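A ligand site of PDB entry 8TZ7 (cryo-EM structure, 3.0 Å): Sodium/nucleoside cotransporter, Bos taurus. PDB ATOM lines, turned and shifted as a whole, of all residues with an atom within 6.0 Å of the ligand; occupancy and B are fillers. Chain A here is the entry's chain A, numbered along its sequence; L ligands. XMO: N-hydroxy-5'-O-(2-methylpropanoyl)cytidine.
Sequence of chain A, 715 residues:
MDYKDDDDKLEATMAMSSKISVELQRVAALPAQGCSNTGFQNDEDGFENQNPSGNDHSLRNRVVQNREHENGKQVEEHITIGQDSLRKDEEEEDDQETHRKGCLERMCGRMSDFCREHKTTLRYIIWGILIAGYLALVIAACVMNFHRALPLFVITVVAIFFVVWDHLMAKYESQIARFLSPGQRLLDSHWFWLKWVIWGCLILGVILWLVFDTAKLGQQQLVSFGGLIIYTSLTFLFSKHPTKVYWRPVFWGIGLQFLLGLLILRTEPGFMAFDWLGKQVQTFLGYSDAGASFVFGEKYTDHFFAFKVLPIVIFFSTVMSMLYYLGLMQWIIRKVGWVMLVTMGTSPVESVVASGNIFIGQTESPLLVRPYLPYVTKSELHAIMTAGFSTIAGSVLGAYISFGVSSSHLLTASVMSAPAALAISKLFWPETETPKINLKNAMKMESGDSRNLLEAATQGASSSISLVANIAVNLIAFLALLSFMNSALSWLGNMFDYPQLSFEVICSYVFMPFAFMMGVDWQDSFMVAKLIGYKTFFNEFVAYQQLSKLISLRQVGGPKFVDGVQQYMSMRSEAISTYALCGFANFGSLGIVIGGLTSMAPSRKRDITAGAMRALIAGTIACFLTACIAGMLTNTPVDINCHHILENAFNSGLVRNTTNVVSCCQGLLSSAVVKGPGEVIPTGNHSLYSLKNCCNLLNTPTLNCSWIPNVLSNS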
ATOM      1  N   PHE A 305     -28.980  17.939  21.652  1.00  0.00           N
ATOM      2  CA  PHE A 305     -28.830  16.620  22.259  1.00  0.00           C
ATOM      3  C   PHE A 305     -29.988  16.311  23.196  1.00  0.00           C
ATOM      4  O   PHE A 305     -30.545  15.203  23.170  1.00  0.00           O
ATOM      5  CB  PHE A 305     -27.505  16.538  23.013  1.00  0.00           C
ATOM      6  CG  PHE A 305     -27.208  15.165  23.538  1.00  0.00           C
ATOM      7  CD1 PHE A 305     -26.591  14.226  22.730  1.00  0.00           C
ATOM      8  CD2 PHE A 305     -27.547  14.815  24.830  1.00  0.00           C
ATOM      9  CE1 PHE A 305     -26.328  12.963  23.212  1.00  0.00           C
ATOM     10  CE2 PHE A 305     -27.282  13.560  25.306  1.00  0.00           C
ATOM     11  CZ  PHE A 305     -26.674  12.631  24.493  1.00  0.00           C
ATOM     12  N   VAL A 309     -31.911  14.361  20.198  1.00  0.00           N
ATOM     13  CA  VAL A 309     -31.262  13.057  20.129  1.00  0.00           C
ATOM     14  C   VAL A 309     -31.904  12.079  21.094  1.00  0.00           C
ATOM     15  O   VAL A 309     -32.278  10.962  20.713  1.00  0.00           O
ATOM     16  CB  VAL A 309     -29.756  13.214  20.406  1.00  0.00           C
ATOM     17  CG1 VAL A 309     -29.054  11.874  20.450  1.00  0.00           C
ATOM     18  CG2 VAL A 309     -29.118  14.105  19.353  1.00  0.00           C
ATOM     19  N   LEU A 310     -32.041  12.461  22.355  1.00  0.00           N
ATOM     20  CA  LEU A 310     -32.526  11.569  23.400  1.00  0.00           C
ATOM     21  C   LEU A 310     -33.953  11.088  23.119  1.00  0.00           C
ATOM     22  O   LEU A 310     -34.262   9.924  23.373  1.00  0.00           O
ATOM     23  CB  LEU A 310     -32.422  12.249  24.759  1.00  0.00           C
ATOM     24  CG  LEU A 310     -31.028  12.201  25.401  1.00  0.00           C
ATOM     25  CD1 LEU A 310     -30.949  13.124  26.611  1.00  0.00           C
ATOM     26  CD2 LEU A 310     -30.646  10.793  25.808  1.00  0.00           C
ATOM     27  N   VAL A 313     -34.305   7.763  21.331  1.00  0.00           N
ATOM     28  CA  VAL A 313     -34.222   6.546  22.118  1.00  0.00           C
ATOM     29  C   VAL A 313     -35.580   6.158  22.684  1.00  0.00           C
ATOM     30  O   VAL A 313     -35.902   4.964  22.740  1.00  0.00           O
ATOM     31  CB  VAL A 313     -33.192   6.726  23.249  1.00  0.00           C
ATOM     32  CG1 VAL A 313     -33.321   5.628  24.283  1.00  0.00           C
ATOM     33  CG2 VAL A 313     -31.768   6.819  22.700  1.00  0.00           C
ATOM     34  N   PHE A 316     -37.539   4.736  19.724  1.00  0.00           N
ATOM     35  CA  PHE A 316     -37.007   3.420  19.393  1.00  0.00           C
ATOM     36  C   PHE A 316     -37.445   2.370  20.400  1.00  0.00           C
ATOM     37  O   PHE A 316     -37.819   1.253  20.019  1.00  0.00           O
ATOM     38  CB  PHE A 316     -35.487   3.486  19.322  1.00  0.00           C
ATOM     39  CG  PHE A 316     -34.832   2.152  19.161  1.00  0.00           C
ATOM     40  CD1 PHE A 316     -34.812   1.526  17.935  1.00  0.00           C
ATOM     41  CD2 PHE A 316     -34.229   1.531  20.236  1.00  0.00           C
ATOM     42  CE1 PHE A 316     -34.207   0.298  17.773  1.00  0.00           C
ATOM     43  CE2 PHE A 316     -33.622   0.307  20.097  1.00  0.00           C
ATOM     44  CZ  PHE A 316     -33.601  -0.312  18.865  1.00  0.00           C
ATOM     45  N   SER A 317     -37.405   2.702  21.693  1.00  0.00           N
ATOM     46  CA  SER A 317     -37.854   1.748  22.711  1.00  0.00           C
ATOM     47  C   SER A 317     -39.327   1.409  22.515  1.00  0.00           C
ATOM     48  O   SER A 317     -39.715   0.232  22.599  1.00  0.00           O
ATOM     49  CB  SER A 317     -37.624   2.324  24.103  1.00  0.00           C
ATOM     50  OG  SER A 317     -36.256   2.574  24.346  1.00  0.00           O
ATOM     51  N   GLY A 361     -30.346  -2.909  22.169  1.00  0.00           N
ATOM     52  CA  GLY A 361     -29.304  -2.393  23.029  1.00  0.00           C
ATOM     53  C   GLY A 361     -28.841  -3.396  24.065  1.00  0.00           C
ATOM     54  O   GLY A 361     -29.428  -4.451  24.281  1.00  0.00           O
ATOM     55  N   GLN A 362     -27.741  -3.028  24.730  1.00  0.00           N
ATOM     56  CA  GLN A 362     -27.152  -3.898  25.733  1.00  0.00           C
ATOM     57  C   GLN A 362     -28.039  -3.999  26.974  1.00  0.00           C
ATOM     58  O   GLN A 362     -28.148  -5.073  27.580  1.00  0.00           O
ATOM     59  CB  GLN A 362     -25.752  -3.383  26.108  1.00  0.00           C
ATOM     60  CG  GLN A 362     -25.736  -1.968  26.646  1.00  0.00           C
ATOM     61  CD  GLN A 362     -24.396  -1.582  27.209  1.00  0.00           C
ATOM     62  OE1 GLN A 362     -23.403  -2.294  27.063  1.00  0.00           O
ATOM     63  NE2 GLN A 362     -24.350  -0.429  27.871  1.00  0.00           N
ATOM     64  N   THR A 363     -28.670  -2.900  27.366  1.00  0.00           N
ATOM     65  CA  THR A 363     -29.501  -2.903  28.564  1.00  0.00           C
ATOM     66  C   THR A 363     -30.731  -3.788  28.395  1.00  0.00           C
ATOM     67  O   THR A 363     -31.169  -4.447  29.343  1.00  0.00           O
ATOM     68  CB  THR A 363     -29.916  -1.479  28.930  1.00  0.00           C
ATOM     69  OG1 THR A 363     -30.449  -0.829  27.770  1.00  0.00           O
ATOM     70  CG2 THR A 363     -28.726  -0.689  29.457  1.00  0.00           C
ATOM     71  N   GLU A 364     -31.296  -3.804  27.184  1.00  0.00           N
ATOM     72  CA  GLU A 364     -32.549  -4.511  26.947  1.00  0.00           C
ATOM     73  C   GLU A 364     -32.362  -5.908  26.352  1.00  0.00           C
ATOM     74  O   GLU A 364     -33.290  -6.715  26.435  1.00  0.00           O
ATOM     75  CB  GLU A 364     -33.450  -3.698  26.015  1.00  0.00           C
ATOM     76  CG  GLU A 364     -33.703  -2.273  26.481  1.00  0.00           C
ATOM     77  CD  GLU A 364     -32.783  -1.258  25.825  1.00  0.00           C
ATOM     78  OE1 GLU A 364     -31.778  -1.660  25.215  1.00  0.00           O
ATOM     79  OE2 GLU A 364     -33.077  -0.044  25.940  1.00  0.00           O
ATOM     80  N   ALA A 393     -26.910  -0.232  19.218  1.00  0.00           N
ATOM     81  CA  ALA A 393     -28.348  -0.334  19.012  1.00  0.00           C
ATOM     82  C   ALA A 393     -28.772   0.352  17.716  1.00  0.00           C
ATOM     83  O   ALA A 393     -27.993   1.057  17.070  1.00  0.00           O
ATOM     84  CB  ALA A 393     -29.093   0.261  20.196  1.00  0.00           C
ATOM     85  N   SER A 395     -31.127   2.654  17.543  1.00  0.00           N
ATOM     86  CA  SER A 395     -31.499   4.049  17.773  1.00  0.00           C
ATOM     87  C   SER A 395     -30.366   4.991  17.367  1.00  0.00           C
ATOM     88  O   SER A 395     -30.607   6.049  16.775  1.00  0.00           O
ATOM     89  CB  SER A 395     -31.857   4.252  19.243  1.00  0.00           C
ATOM     90  OG  SER A 395     -30.831   3.750  20.081  1.00  0.00           O
ATOM     91  N   VAL A 396     -29.130   4.632  17.702  1.00  0.00           N
ATOM     92  CA  VAL A 396     -27.985   5.486  17.416  1.00  0.00           C
ATOM     93  C   VAL A 396     -27.621   5.473  15.937  1.00  0.00           C
ATOM     94  O   VAL A 396     -26.882   6.361  15.482  1.00  0.00           O
ATOM     95  CB  VAL A 396     -26.793   5.040  18.278  1.00  0.00           C
ATOM     96  CG1 VAL A 396     -27.193   4.983  19.740  1.00  0.00           C
ATOM     97  CG2 VAL A 396     -26.280   3.684  17.818  1.00  0.00           C
ATOM     98  N   ALA A 399     -28.715   8.683  13.921  1.00  0.00           N
ATOM     99  CA  ALA A 399     -27.889   9.828  14.270  1.00  0.00           C
ATOM    100  C   ALA A 399     -26.511   9.715  13.650  1.00  0.00           C
ATOM    101  O   ALA A 399     -25.994  10.679  13.055  1.00  0.00           O
ATOM    102  CB  ALA A 399     -27.790   9.941  15.788  1.00  0.00           C
ATOM    103  N   TYR A 400     -25.881   8.543  13.778  1.00  0.00           N
ATOM    104  CA  TYR A 400     -24.522   8.393  13.275  1.00  0.00           C
ATOM    105  C   TYR A 400     -24.464   8.503  11.753  1.00  0.00           C
ATOM    106  O   TYR A 400     -23.513   9.055  11.200  1.00  0.00           O
ATOM    107  CB  TYR A 400     -23.933   7.070  13.752  1.00  0.00           C
ATOM    108  CG  TYR A 400     -23.771   6.987  15.268  1.00  0.00           C
ATOM    109  CD1 TYR A 400     -23.705   8.141  16.037  1.00  0.00           C
ATOM    110  CD2 TYR A 400     -23.689   5.771  15.918  1.00  0.00           C
ATOM    111  CE1 TYR A 400     -23.561   8.079  17.407  1.00  0.00           C
ATOM    112  CE2 TYR A 400     -23.546   5.701  17.293  1.00  0.00           C
ATOM    113  CZ  TYR A 400     -23.483   6.854  18.027  1.00  0.00           C
ATOM    114  OH  TYR A 400     -23.349   6.795  19.397  1.00  0.00           O
ATOM    115  N   LEU A 467     -33.153   5.490  31.347  1.00  0.00           N
ATOM    116  CA  LEU A 467     -31.979   5.430  30.488  1.00  0.00           C
ATOM    117  C   LEU A 467     -31.528   6.820  30.058  1.00  0.00           C
ATOM    118  O   LEU A 467     -30.342   7.153  30.123  1.00  0.00           O
ATOM    119  CB  LEU A 467     -32.284   4.556  29.269  1.00  0.00           C
ATOM    120  CG  LEU A 467     -31.173   4.409  28.225  1.00  0.00           C
ATOM    121  CD1 LEU A 467     -29.974   3.698  28.823  1.00  0.00           C
ATOM    122  CD2 LEU A 467     -31.714   3.677  27.021  1.00  0.00           C
ATOM    123  N   ILE A 471     -27.970   8.637  30.924  1.00  0.00           N
ATOM    124  CA  ILE A 471     -27.083   9.035  29.836  1.00  0.00           C
ATOM    125  C   ILE A 471     -26.712  10.508  29.971  1.00  0.00           C
ATOM    126  O   ILE A 471     -25.530  10.877  29.914  1.00  0.00           O
ATOM    127  CB  ILE A 471     -27.743   8.756  28.482  1.00  0.00           C
ATOM    128  CG1 ILE A 471     -27.884   7.251  28.243  1.00  0.00           C
ATOM    129  CG2 ILE A 471     -26.964   9.413  27.337  1.00  0.00           C
ATOM    130  CD1 ILE A 471     -28.621   6.910  26.961  1.00  0.00           C
ATOM    131  N   LEU A 475     -22.943  11.947  30.817  1.00  0.00           N
ATOM    132  CA  LEU A 475     -22.272  12.810  29.851  1.00  0.00           C
ATOM    133  C   LEU A 475     -21.839  14.120  30.494  1.00  0.00           C
ATOM    134  O   LEU A 475     -20.695  14.554  30.313  1.00  0.00           O
ATOM    135  CB  LEU A 475     -23.199  13.079  28.658  1.00  0.00           C
ATOM    136  CG  LEU A 475     -22.994  12.117  27.499  1.00  0.00           C
ATOM    137  CD1 LEU A 475     -24.165  12.185  26.548  1.00  0.00           C
ATOM    138  CD2 LEU A 475     -21.708  12.463  26.793  1.00  0.00           C
ATOM    139  N   ASN A 539     -18.008   7.911  25.717  1.00  0.00           N
ATOM    140  CA  ASN A 539     -18.793   7.040  24.860  1.00  0.00           C
ATOM    141  C   ASN A 539     -18.409   7.279  23.388  1.00  0.00           C
ATOM    142  O   ASN A 539     -17.594   8.136  23.062  1.00  0.00           O
ATOM    143  CB  ASN A 539     -20.287   7.241  25.099  1.00  0.00           C
ATOM    144  CG  ASN A 539     -20.669   8.708  25.170  1.00  0.00           C
ATOM    145  OD1 ASN A 539     -20.252   9.520  24.344  1.00  0.00           O
ATOM    146  ND2 ASN A 539     -21.459   9.054  26.154  1.00  0.00           N
ATOM    147  N   GLU A 540     -18.989   6.472  22.504  1.00  0.00           N
ATOM    148  CA  GLU A 540     -18.649   6.520  21.087  1.00  0.00           C
ATOM    149  C   GLU A 540     -19.386   7.620  20.340  1.00  0.00           C
ATOM    150  O   GLU A 540     -19.067   7.873  19.169  1.00  0.00           O
ATOM    151  CB  GLU A 540     -18.940   5.160  20.436  1.00  0.00           C
ATOM    152  CG  GLU A 540     -20.413   4.845  20.186  1.00  0.00           C
ATOM    153  CD  GLU A 540     -21.193   4.597  21.468  1.00  0.00           C
ATOM    154  OE1 GLU A 540     -20.559   4.305  22.507  1.00  0.00           O
ATOM    155  OE2 GLU A 540     -22.437   4.681  21.436  1.00  0.00           O
ATOM    156  N   PHE A 541     -20.347   8.286  20.981  1.00  0.00           N
ATOM    157  CA  PHE A 541     -21.031   9.402  20.335  1.00  0.00           C
ATOM    158  C   PHE A 541     -20.072  10.549  20.060  1.00  0.00           C
ATOM    159  O   PHE A 541     -20.039  11.094  18.947  1.00  0.00           O
ATOM    160  CB  PHE A 541     -22.186   9.854  21.227  1.00  0.00           C
ATOM    161  CG  PHE A 541     -23.008  10.973  20.646  1.00  0.00           C
ATOM    162  CD1 PHE A 541     -22.675  12.294  20.908  1.00  0.00           C
ATOM    163  CD2 PHE A 541     -24.116  10.713  19.871  1.00  0.00           C
ATOM    164  CE1 PHE A 541     -23.437  13.325  20.387  1.00  0.00           C
ATOM    165  CE2 PHE A 541     -24.870  11.736  19.342  1.00  0.00           C
ATOM    166  CZ  PHE A 541     -24.529  13.047  19.608  1.00  0.00           C
ATOM    167  N   GLY A 583     -19.247   0.286  18.795  1.00  0.00           N
ATOM    168  CA  GLY A 583     -19.481  -0.488  20.000  1.00  0.00           C
ATOM    169  C   GLY A 583     -20.015   0.372  21.128  1.00  0.00           C
ATOM    170  O   GLY A 583     -19.982   1.603  21.086  1.00  0.00           O
ATOM    171  N   PHE A 584     -20.515  -0.323  22.151  1.00  0.00           N
ATOM    172  CA  PHE A 584     -20.974   0.298  23.391  1.00  0.00           C
ATOM    173  C   PHE A 584     -19.998   0.040  24.541  1.00  0.00           C
ATOM    174  O   PHE A 584     -20.376   0.166  25.710  1.00  0.00           O
ATOM    175  CB  PHE A 584     -22.363  -0.220  23.770  1.00  0.00           C
ATOM    176  CG  PHE A 584     -23.512   0.475  23.073  1.00  0.00           C
ATOM    177  CD1 PHE A 584     -23.308   1.492  22.164  1.00  0.00           C
ATOM    178  CD2 PHE A 584     -24.810   0.100  23.358  1.00  0.00           C
ATOM    179  CE1 PHE A 584     -24.372   2.119  21.544  1.00  0.00           C
ATOM    180  CE2 PHE A 584     -25.885   0.721  22.744  1.00  0.00           C
ATOM    181  CZ  PHE A 584     -25.660   1.733  21.834  1.00  0.00           C
ATOM    182  N   ASN A 586     -17.549   1.221  26.707  1.00  0.00           N
ATOM    183  CA  ASN A 586     -16.878   2.333  27.360  1.00  0.00           C
ATOM    184  C   ASN A 586     -16.889   2.100  28.858  1.00  0.00           C
ATOM    185  O   ASN A 586     -17.799   1.455  29.393  1.00  0.00           O
ATOM    186  CB  ASN A 586     -17.521   3.683  27.013  1.00  0.00           C
ATOM    187  CG  ASN A 586     -19.028   3.679  27.223  1.00  0.00           C
ATOM    188  OD1 ASN A 586     -19.764   2.993  26.513  1.00  0.00           O
ATOM    189  ND2 ASN A 586     -19.495   4.489  28.174  1.00  0.00           N
ATOM    190  N   SER A 589     -19.821   3.010  30.911  1.00  0.00           N
ATOM    191  CA  SER A 589     -20.946   2.111  30.692  1.00  0.00           C
ATOM    192  C   SER A 589     -20.835   0.791  31.445  1.00  0.00           C
ATOM    193  O   SER A 589     -21.786   0.013  31.426  1.00  0.00           O
ATOM    194  CB  SER A 589     -21.087   1.828  29.190  1.00  0.00           C
ATOM    195  OG  SER A 589     -22.241   1.061  28.923  1.00  0.00           O
ATOM    196  N   ILE A 592     -23.686   0.520  34.284  1.00  0.00           N
ATOM    197  CA  ILE A 592     -25.091   0.341  33.926  1.00  0.00           C
ATOM    198  C   ILE A 592     -25.366  -1.114  33.559  1.00  0.00           C
ATOM    199  O   ILE A 592     -26.405  -1.667  33.922  1.00  0.00           O
ATOM    200  CB  ILE A 592     -25.486   1.307  32.801  1.00  0.00           C
ATOM    201  CG1 ILE A 592     -24.594   1.120  31.573  1.00  0.00           C
ATOM    202  CG2 ILE A 592     -25.389   2.742  33.295  1.00  0.00           C
ATOM    203  CD1 ILE A 592     -25.055   1.895  30.360  1.00  0.00           C
HETATM  204  C10 XMO L   1     -24.451   3.486  25.558  1.00  0.00           C
HETATM  205  C11 XMO L   1     -25.492   3.907  26.188  1.00  0.00           C
HETATM  206  C01 XMO L   1     -27.080   8.500  21.027  1.00  0.00           C
HETATM  207  C02 XMO L   1     -27.315   8.228  22.514  1.00  0.00           C
HETATM  208  C03 XMO L   1     -28.344   9.155  23.075  1.00  0.00           C
HETATM  209  C04 XMO L   1     -25.996   8.298  23.325  1.00  0.00           C
HETATM  210  C07 XMO L   1     -24.382   7.221  24.851  1.00  0.00           C
HETATM  211  C08 XMO L   1     -24.325   5.948  25.694  1.00  0.00           C
HETATM  212  C09 XMO L   1     -23.824   4.758  24.826  1.00  0.00           C
HETATM  213  C14 XMO L   1     -27.406   4.115  24.586  1.00  0.00           C
HETATM  214  C15 XMO L   1     -28.649   3.565  23.967  1.00  0.00           C
HETATM  215  C16 XMO L   1     -29.160   2.229  24.410  1.00  0.00           C
HETATM  216  C18 XMO L   1     -27.211   2.029  26.047  1.00  0.00           C
HETATM  217  N13 XMO L   1     -26.692   3.355  25.610  1.00  0.00           N
HETATM  218  N17 XMO L   1     -28.455   1.479  25.428  1.00  0.00           N
HETATM  219  N20 XMO L   1     -30.358   1.693  23.820  1.00  0.00           N
HETATM  220  O05 XMO L   1     -25.483   9.312  23.537  1.00  0.00           O
HETATM  221  O06 XMO L   1     -25.404   7.034  23.833  1.00  0.00           O
HETATM  222  O12 XMO L   1     -25.520   5.587  26.070  1.00  0.00           O
HETATM  223  O19 XMO L   1     -26.648   1.424  26.861  1.00  0.00           O
HETATM  224  O21 XMO L   1     -31.052   2.447  22.809  1.00  0.00           O
HETATM  225  O22 XMO L   1     -23.486   2.940  26.514  1.00  0.00           O
HETATM  226  O23 XMO L   1     -22.507   4.693  24.828  1.00  0.00           O
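An oxygen (O21) of the ligand lies within hydrogen-bond range of the side-chain hydroxyl (OG) of Ser 395, 3.0 Å away.
OE1 of Glu 540 lies within hydrogen-bond range of O23 of the ligand (3.1 Å).
The side-chain hydroxyl (OG) of Ser 589 is in hydrogen-bond range of an oxygen (O22) of the ligand (3.3 Å).
NE2 of Gln 362 is in hydrogen-bond range of O19 of the ligand (3.1 Å).
The backbone carbonyl oxygen (O) of Phe 584 lies close to the side-chain amide oxygen (OD1) of Asn 586 (3.0 Å).
OG1 of Thr 363 is in hydrogen-bond range of OE1 of Glu 364 (3.0 Å).
The side-chain amide nitrogen (NE2) of Gln 362 is in hydrogen-bond range of the side-chain hydroxyl (OG) of Ser 589 (2.8 Å).
The side-chain hydroxyl of Tyr 400 sits at hydrogen-bond distance from the side-chain carboxylate of Glu 540 (3.1 Å).
The side-chain amide nitrogen (ND2) of Asn 586 lies close to the backbone NH (N) of Ser 589, 3.1 Å away.
O of Phe 305 sits at hydrogen-bond distance from N of Leu 310 (3.2 Å).
Residues that only touch the ligand: Phe 305 (3.7 Å), Val 309 (3.8 Å), Leu 310 (3.9 Å), Thr 363 (3.8 Å), Glu 364 (3.9 Å), Ala 393 (3.9 Å), Val 396 (3.7 Å), Leu 467 (3.9 Å), Ile 471 (3.5 Å), Asn 539 (3.4 Å), Phe 541 (3.9 Å), Phe 584 (3.8 Å), Asn 586 (3.6 Å) and Ile 592 (3.9 Å).
Hydrophobic or aromatic side chains within 4 Å of the ligand: Phe 305, Val 309, Leu 310, Ala 393, Val 396, Leu 467, Ile 471, Phe 541, Phe 584 and Ile 592.
18 residues have an atom within 4 Å of the ligand: Phe 305, Val 309, Leu 310, Gln 362, Thr 363, Glu 364, Ala 393, Ser 395, Val 396, Leu 467, Ile 471, Asn 539, Glu 540, Phe 541, Phe 584, Asn 586, Ser 589 and Ile 592.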
